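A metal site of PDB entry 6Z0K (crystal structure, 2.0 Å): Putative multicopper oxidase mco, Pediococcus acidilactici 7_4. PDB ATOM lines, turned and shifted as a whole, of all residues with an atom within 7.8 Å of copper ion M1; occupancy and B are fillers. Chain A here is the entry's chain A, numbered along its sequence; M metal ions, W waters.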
ATOM      1  N   HIS A 105     -23.459 -33.450  -2.903  1.00  0.00           N
ATOM      2  CA  HIS A 105     -22.916 -32.890  -4.163  1.00  0.00           C
ATOM      3  C   HIS A 105     -21.421 -33.198  -4.289  1.00  0.00           C
ATOM      4  O   HIS A 105     -20.648 -32.786  -3.406  1.00  0.00           O
ATOM      5  CB  HIS A 105     -23.136 -31.386  -4.277  1.00  0.00           C
ATOM      6  CG  HIS A 105     -22.603 -30.821  -5.550  1.00  0.00           C
ATOM      7  ND1 HIS A 105     -22.993 -31.292  -6.794  1.00  0.00           N
ATOM      8  CD2 HIS A 105     -21.684 -29.858  -5.789  1.00  0.00           C
ATOM      9  CE1 HIS A 105     -22.360 -30.633  -7.731  1.00  0.00           C
ATOM     10  NE2 HIS A 105     -21.544 -29.756  -7.142  1.00  0.00           N
ATOM     11  N   TRP A 106     -21.041 -33.867  -5.378  1.00  0.00           N
ATOM     12  CA  TRP A 106     -19.626 -34.140  -5.709  1.00  0.00           C
ATOM     13  C   TRP A 106     -19.101 -32.983  -6.544  1.00  0.00           C
ATOM     14  O   TRP A 106     -19.156 -33.045  -7.795  1.00  0.00           O
ATOM     15  CB  TRP A 106     -19.509 -35.504  -6.404  1.00  0.00           C
ATOM     16  CG  TRP A 106     -20.194 -36.596  -5.661  1.00  0.00           C
ATOM     17  CD1 TRP A 106     -21.482 -37.020  -5.831  1.00  0.00           C
ATOM     18  CD2 TRP A 106     -19.659 -37.377  -4.578  1.00  0.00           C
ATOM     19  NE1 TRP A 106     -21.778 -38.029  -4.950  1.00  0.00           N
ATOM     20  CE2 TRP A 106     -20.667 -38.278  -4.176  1.00  0.00           C
ATOM     21  CE3 TRP A 106     -18.420 -37.427  -3.927  1.00  0.00           C
ATOM     22  CZ2 TRP A 106     -20.485 -39.207  -3.148  1.00  0.00           C
ATOM     23  CZ3 TRP A 106     -18.227 -38.342  -2.916  1.00  0.00           C
ATOM     24  CH2 TRP A 106     -19.253 -39.219  -2.529  1.00  0.00           C
ATOM     25  N   HIS A 107     -18.643 -31.928  -5.875  1.00  0.00           N
ATOM     26  CA  HIS A 107     -18.169 -30.681  -6.531  1.00  0.00           C
ATOM     27  C   HIS A 107     -16.945 -31.026  -7.386  1.00  0.00           C
ATOM     28  O   HIS A 107     -15.878 -31.321  -6.810  1.00  0.00           O
ATOM     29  CB  HIS A 107     -17.874 -29.580  -5.512  1.00  0.00           C
ATOM     30  CG  HIS A 107     -17.338 -28.334  -6.115  1.00  0.00           C
ATOM     31  ND1 HIS A 107     -17.984 -27.118  -6.001  1.00  0.00           N
ATOM     32  CD2 HIS A 107     -16.239 -28.101  -6.859  1.00  0.00           C
ATOM     33  CE1 HIS A 107     -17.300 -26.192  -6.629  1.00  0.00           C
ATOM     34  NE2 HIS A 107     -16.214 -26.769  -7.165  1.00  0.00           N
ATOM     35  N   GLY A 108     -17.101 -30.941  -8.704  1.00  0.00           N
ATOM     36  CA  GLY A 108     -16.009 -31.135  -9.678  1.00  0.00           C
ATOM     37  C   GLY A 108     -16.112 -32.446 -10.414  1.00  0.00           C
ATOM     38  O   GLY A 108     -15.315 -32.667 -11.342  1.00  0.00           O
ATOM     39  N   TRP A 144     -14.250 -32.318  -4.195  1.00  0.00           N
ATOM     40  CA  TRP A 144     -14.761 -32.471  -2.812  1.00  0.00           C
ATOM     41  C   TRP A 144     -16.246 -32.801  -2.789  1.00  0.00           C
ATOM     42  O   TRP A 144     -16.919 -32.634  -3.822  1.00  0.00           O
ATOM     43  CB  TRP A 144     -14.436 -31.248  -1.934  1.00  0.00           C
ATOM     44  CG  TRP A 144     -14.870 -29.915  -2.449  1.00  0.00           C
ATOM     45  CD1 TRP A 144     -14.703 -29.387  -3.691  1.00  0.00           C
ATOM     46  CD2 TRP A 144     -15.487 -28.882  -1.649  1.00  0.00           C
ATOM     47  NE1 TRP A 144     -15.195 -28.106  -3.731  1.00  0.00           N
ATOM     48  CE2 TRP A 144     -15.691 -27.772  -2.502  1.00  0.00           C
ATOM     49  CE3 TRP A 144     -15.892 -28.796  -0.320  1.00  0.00           C
ATOM     50  CZ2 TRP A 144     -16.281 -26.592  -2.054  1.00  0.00           C
ATOM     51  CZ3 TRP A 144     -16.483 -27.638   0.126  1.00  0.00           C
ATOM     52  CH2 TRP A 144     -16.676 -26.546  -0.735  1.00  0.00           C
ATOM     53  N   LEU A 145     -16.706 -33.257  -1.631  1.00  0.00           N
ATOM     54  CA  LEU A 145     -18.126 -33.571  -1.362  1.00  0.00           C
ATOM     55  C   LEU A 145     -18.649 -32.576  -0.331  1.00  0.00           C
ATOM     56  O   LEU A 145     -17.946 -32.328   0.665  1.00  0.00           O
ATOM     57  CB  LEU A 145     -18.247 -35.003  -0.831  1.00  0.00           C
ATOM     58  CG  LEU A 145     -19.571 -35.304  -0.115  1.00  0.00           C
ATOM     59  CD1 LEU A 145     -20.717 -35.352  -1.111  1.00  0.00           C
ATOM     60  CD2 LEU A 145     -19.492 -36.594   0.673  1.00  0.00           C
ATOM     61  N   HIS A 146     -19.830 -32.029  -0.570  1.00  0.00           N
ATOM     62  CA  HIS A 146     -20.537 -31.163   0.400  1.00  0.00           C
ATOM     63  C   HIS A 146     -22.027 -31.130   0.075  1.00  0.00           C
ATOM     64  O   HIS A 146     -22.442 -31.523  -1.013  1.00  0.00           O
ATOM     65  CB  HIS A 146     -19.872 -29.782   0.473  1.00  0.00           C
ATOM     66  CG  HIS A 146     -20.099 -28.976  -0.747  1.00  0.00           C
ATOM     67  ND1 HIS A 146     -21.323 -28.419  -1.042  1.00  0.00           N
ATOM     68  CD2 HIS A 146     -19.279 -28.635  -1.758  1.00  0.00           C
ATOM     69  CE1 HIS A 146     -21.246 -27.757  -2.179  1.00  0.00           C
ATOM     70  NE2 HIS A 146     -20.001 -27.886  -2.642  1.00  0.00           N
ATOM     71  N   PRO A 147     -22.875 -30.677   1.034  1.00  0.00           N
ATOM     72  CA  PRO A 147     -24.320 -30.647   0.840  1.00  0.00           C
ATOM     73  C   PRO A 147     -24.767 -29.532  -0.117  1.00  0.00           C
ATOM     74  O   PRO A 147     -24.054 -28.551  -0.233  1.00  0.00           O
ATOM     75  CB  PRO A 147     -24.883 -30.415   2.252  1.00  0.00           C
ATOM     76  CG  PRO A 147     -23.752 -29.747   3.008  1.00  0.00           C
ATOM     77  CD  PRO A 147     -22.469 -30.203   2.356  1.00  0.00           C
ATOM     78  N   HIS A 148     -25.911 -29.714  -0.761  1.00  0.00           N
ATOM     79  CA  HIS A 148     -26.469 -28.700  -1.699  1.00  0.00           C
ATOM     80  C   HIS A 148     -27.985 -28.519  -1.547  1.00  0.00           C
ATOM     81  O   HIS A 148     -28.655 -28.226  -2.528  1.00  0.00           O
ATOM     82  CB  HIS A 148     -26.079 -29.097  -3.127  1.00  0.00           C
ATOM     83  CG  HIS A 148     -25.702 -27.941  -3.971  1.00  0.00           C
ATOM     84  ND1 HIS A 148     -26.553 -26.887  -4.201  1.00  0.00           N
ATOM     85  CD2 HIS A 148     -24.561 -27.673  -4.655  1.00  0.00           C
ATOM     86  CE1 HIS A 148     -25.968 -26.018  -4.993  1.00  0.00           C
ATOM     87  NE2 HIS A 148     -24.749 -26.472  -5.286  1.00  0.00           N
ATOM     88  N   THR A 153     -27.662 -24.643   2.300  1.00  0.00           N
ATOM     89  CA  THR A 153     -26.299 -25.127   1.937  1.00  0.00           C
ATOM     90  C   THR A 153     -25.245 -24.460   2.837  1.00  0.00           C
ATOM     91  O   THR A 153     -24.407 -25.186   3.381  1.00  0.00           O
ATOM     92  CB  THR A 153     -26.018 -24.898   0.450  1.00  0.00           C
ATOM     93  OG1 THR A 153     -26.950 -25.674  -0.299  1.00  0.00           O
ATOM     94  CG2 THR A 153     -24.602 -25.284   0.070  1.00  0.00           C
ATOM     95  N   VAL A 157     -22.793 -26.603   5.499  1.00  0.00           N
ATOM     96  CA  VAL A 157     -21.309 -26.578   5.359  1.00  0.00           C
ATOM     97  C   VAL A 157     -20.708 -25.990   6.640  1.00  0.00           C
ATOM     98  O   VAL A 157     -19.731 -26.570   7.156  1.00  0.00           O
ATOM     99  CB  VAL A 157     -20.843 -25.810   4.108  1.00  0.00           C
ATOM    100  CG1 VAL A 157     -19.337 -25.599   4.115  1.00  0.00           C
ATOM    101  CG2 VAL A 157     -21.265 -26.539   2.837  1.00  0.00           C
ATOM    102  N   LEU A 238      -7.777 -26.536  -0.587  1.00  0.00           N
ATOM    103  CA  LEU A 238      -9.196 -26.313  -0.970  1.00  0.00           C
ATOM    104  C   LEU A 238      -9.709 -25.133  -0.136  1.00  0.00           C
ATOM    105  O   LEU A 238      -9.609 -25.205   1.100  1.00  0.00           O
ATOM    106  CB  LEU A 238     -10.017 -27.569  -0.687  1.00  0.00           C
ATOM    107  CG  LEU A 238     -11.523 -27.364  -0.434  1.00  0.00           C
ATOM    108  CD1 LEU A 238     -12.222 -26.775  -1.649  1.00  0.00           C
ATOM    109  CD2 LEU A 238     -12.184 -28.672  -0.046  1.00  0.00           C
ATOM    110  N   CYS A 279     -13.638 -19.015  -3.049  1.00  0.00           N
ATOM    111  CA  CYS A 279     -14.423 -20.159  -2.534  1.00  0.00           C
ATOM    112  C   CYS A 279     -14.489 -21.292  -3.562  1.00  0.00           C
ATOM    113  O   CYS A 279     -14.777 -21.012  -4.742  1.00  0.00           O
ATOM    114  CB  CYS A 279     -15.833 -19.725  -2.138  1.00  0.00           C
ATOM    115  SG  CYS A 279     -15.839 -18.562  -0.762  1.00  0.00           S
ATOM    116  N   ALA A 280     -14.187 -22.513  -3.116  1.00  0.00           N
ATOM    117  CA  ALA A 280     -14.303 -23.796  -3.854  1.00  0.00           C
ATOM    118  C   ALA A 280     -13.127 -24.029  -4.813  1.00  0.00           C
ATOM    119  O   ALA A 280     -13.082 -25.121  -5.410  1.00  0.00           O
ATOM    120  CB  ALA A 280     -15.610 -23.872  -4.600  1.00  0.00           C
ATOM    121  N   ARG A 282      -9.375 -25.036  -5.868  1.00  0.00           N
ATOM    122  CA  ARG A 282      -8.318 -25.932  -5.356  1.00  0.00           C
ATOM    123  C   ARG A 282      -6.997 -25.585  -6.027  1.00  0.00           C
ATOM    124  O   ARG A 282      -7.008 -25.174  -7.210  1.00  0.00           O
ATOM    125  CB  ARG A 282      -8.657 -27.404  -5.600  1.00  0.00           C
ATOM    126  CG  ARG A 282      -9.719 -27.966  -4.664  1.00  0.00           C
ATOM    127  CD  ARG A 282     -11.116 -27.736  -5.209  1.00  0.00           C
ATOM    128  NE  ARG A 282     -11.407 -28.583  -6.369  1.00  0.00           N
ATOM    129  CZ  ARG A 282     -12.339 -28.356  -7.285  1.00  0.00           C
ATOM    130  NH1 ARG A 282     -12.503 -29.211  -8.275  1.00  0.00           N
ATOM    131  NH2 ARG A 282     -13.111 -27.287  -7.213  1.00  0.00           N
ATOM    132  N   HIS A 393     -19.147 -20.926 -10.467  1.00  0.00           N
ATOM    133  CA  HIS A 393     -19.004 -22.404 -10.557  1.00  0.00           C
ATOM    134  C   HIS A 393     -20.093 -23.009 -11.444  1.00  0.00           C
ATOM    135  O   HIS A 393     -21.251 -22.565 -11.332  1.00  0.00           O
ATOM    136  CB  HIS A 393     -19.022 -23.029  -9.155  1.00  0.00           C
ATOM    137  CG  HIS A 393     -19.157 -24.510  -9.150  1.00  0.00           C
ATOM    138  ND1 HIS A 393     -18.224 -25.344  -9.734  1.00  0.00           N
ATOM    139  CD2 HIS A 393     -20.099 -25.318  -8.634  1.00  0.00           C
ATOM    140  CE1 HIS A 393     -18.590 -26.597  -9.581  1.00  0.00           C
ATOM    141  NE2 HIS A 393     -19.741 -26.607  -8.915  1.00  0.00           N
ATOM    142  N   HIS A 395     -21.750 -26.841 -12.470  1.00  0.00           N
ATOM    143  CA  HIS A 395     -21.871 -28.291 -12.163  1.00  0.00           C
ATOM    144  C   HIS A 395     -21.642 -29.128 -13.420  1.00  0.00           C
ATOM    145  O   HIS A 395     -21.850 -28.622 -14.537  1.00  0.00           O
ATOM    146  CB  HIS A 395     -23.246 -28.626 -11.583  1.00  0.00           C
ATOM    147  CG  HIS A 395     -23.448 -28.160 -10.182  1.00  0.00           C
ATOM    148  ND1 HIS A 395     -24.326 -28.802  -9.327  1.00  0.00           N
ATOM    149  CD2 HIS A 395     -22.918 -27.136  -9.480  1.00  0.00           C
ATOM    150  CE1 HIS A 395     -24.319 -28.198  -8.163  1.00  0.00           C
ATOM    151  NE2 HIS A 395     -23.460 -27.171  -8.227  1.00  0.00           N
ATOM    152  N   ASP A 418     -13.307 -25.646 -12.653  1.00  0.00           N
ATOM    153  CA  ASP A 418     -14.783 -25.674 -12.469  1.00  0.00           C
ATOM    154  C   ASP A 418     -15.253 -24.457 -11.671  1.00  0.00           C
ATOM    155  O   ASP A 418     -16.471 -24.270 -11.575  1.00  0.00           O
ATOM    156  CB  ASP A 418     -15.252 -26.988 -11.837  1.00  0.00           C
ATOM    157  CG  ASP A 418     -14.710 -27.259 -10.443  1.00  0.00           C
ATOM    158  OD1 ASP A 418     -14.733 -26.324  -9.616  1.00  0.00           O
ATOM    159  OD2 ASP A 418     -14.290 -28.401 -10.195  1.00  0.00           O
ATOM    160  N   THR A 419     -14.331 -23.666 -11.104  1.00  0.00           N
ATOM    161  CA  THR A 419     -14.664 -22.455 -10.323  1.00  0.00           C
ATOM    162  C   THR A 419     -13.652 -21.350 -10.647  1.00  0.00           C
ATOM    163  O   THR A 419     -12.436 -21.621 -10.569  1.00  0.00           O
ATOM    164  CB  THR A 419     -14.694 -22.737  -8.817  1.00  0.00           C
ATOM    165  OG1 THR A 419     -15.511 -23.884  -8.557  1.00  0.00           O
ATOM    166  CG2 THR A 419     -15.203 -21.559  -8.024  1.00  0.00           C
ATOM    167  N   HIS A 443     -23.676 -21.053 -10.534  1.00  0.00           N
ATOM    168  CA  HIS A 443     -23.918 -20.093  -9.431  1.00  0.00           C
ATOM    169  C   HIS A 443     -22.613 -19.521  -8.897  1.00  0.00           C
ATOM    170  O   HIS A 443     -21.529 -20.047  -9.208  1.00  0.00           O
ATOM    171  CB  HIS A 443     -24.676 -20.790  -8.295  1.00  0.00           C
ATOM    172  CG  HIS A 443     -23.986 -21.985  -7.737  1.00  0.00           C
ATOM    173  ND1 HIS A 443     -23.192 -21.916  -6.605  1.00  0.00           N
ATOM    174  CD2 HIS A 443     -23.970 -23.270  -8.133  1.00  0.00           C
ATOM    175  CE1 HIS A 443     -22.721 -23.110  -6.333  1.00  0.00           C
ATOM    176  NE2 HIS A 443     -23.178 -23.967  -7.254  1.00  0.00           N
ATOM    177  N   HIS A 445     -20.230 -19.233  -5.728  1.00  0.00           N
ATOM    178  CA  HIS A 445     -19.893 -20.201  -4.661  1.00  0.00           C
ATOM    179  C   HIS A 445     -19.617 -19.509  -3.326  1.00  0.00           C
ATOM    180  O   HIS A 445     -19.152 -20.192  -2.398  1.00  0.00           O
ATOM    181  CB  HIS A 445     -18.726 -21.103  -5.065  1.00  0.00           C
ATOM    182  CG  HIS A 445     -18.858 -22.471  -4.490  1.00  0.00           C
ATOM    183  ND1 HIS A 445     -18.604 -22.730  -3.151  1.00  0.00           N
ATOM    184  CD2 HIS A 445     -19.249 -23.640  -5.039  1.00  0.00           C
ATOM    185  CE1 HIS A 445     -18.812 -24.016  -2.915  1.00  0.00           C
ATOM    186  NE2 HIS A 445     -19.210 -24.580  -4.050  1.00  0.00           N
ATOM    187  N   LEU A 447     -21.458 -19.042  -0.398  1.00  0.00           N
ATOM    188  CA  LEU A 447     -22.620 -19.931  -0.100  1.00  0.00           C
ATOM    189  C   LEU A 447     -23.858 -19.116   0.295  1.00  0.00           C
ATOM    190  O   LEU A 447     -24.968 -19.584  -0.018  1.00  0.00           O
ATOM    191  CB  LEU A 447     -22.217 -20.946   0.976  1.00  0.00           C
ATOM    192  CG  LEU A 447     -21.104 -21.915   0.582  1.00  0.00           C
ATOM    193  CD1 LEU A 447     -20.770 -22.845   1.735  1.00  0.00           C
ATOM    194  CD2 LEU A 447     -21.472 -22.737  -0.656  1.00  0.00           C
ATOM    195  N   GLU A 450     -25.379 -17.942  -2.992  1.00  0.00           N
ATOM    196  CA  GLU A 450     -26.039 -19.143  -3.560  1.00  0.00           C
ATOM    197  C   GLU A 450     -27.402 -19.323  -2.892  1.00  0.00           C
ATOM    198  O   GLU A 450     -28.410 -19.452  -3.625  1.00  0.00           O
ATOM    199  CB  GLU A 450     -25.126 -20.355  -3.329  1.00  0.00           C
ATOM    200  CG  GLU A 450     -25.690 -21.672  -3.819  1.00  0.00           C
ATOM    201  CD  GLU A 450     -24.925 -22.856  -3.256  1.00  0.00           C
ATOM    202  OE1 GLU A 450     -25.582 -23.857  -2.889  1.00  0.00           O
ATOM    203  OE2 GLU A 450     -23.686 -22.777  -3.178  1.00  0.00           O
HETATM  204 CU    CU M   1     -19.351 -26.777  -4.444  1.00  0.00          CU
HETATM  205 CU    CU M   2     -20.555 -28.077  -7.817  1.00  0.00          CU
HETATM  206 CU    CU M   3     -23.457 -25.950  -6.728  1.00  0.00          CU
HETATM  207  O   HOH W   1     -21.486 -26.536  -5.588  1.00  0.00           O
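N of His 107 lies within hydrogen-bond range of O of Trp 144. NE2 of His 107 lies within hydrogen-bond range of OG1 of Thr 419, at 3.3 Å. The guanidinium group (NH2) of Arg 282 sits at hydrogen-bond distance from a ring nitrogen (NE2) of His 107, 3.1 Å away. NE2 of His 107 lies within hydrogen-bond range of OD1 of Asp 418 (2.9 Å). O of His 146 is in hydrogen-bond range of N of His 105 (2.9 Å).
Trp 144 touches copper ion M1 (CZ2 to CU, 3.9 Å). Four residues have an atom within 4 Å of copper ion M1: His 107, Trp 144, His 146 and His 445.
Copper ion M1 is bound by a ring nitrogen (ND1) of His 107, a ring nitrogen (NE2) of His 146, a ring nitrogen (NE2) of His 445 and water W1. Copper ion M1 has four donor atoms within binding distance.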
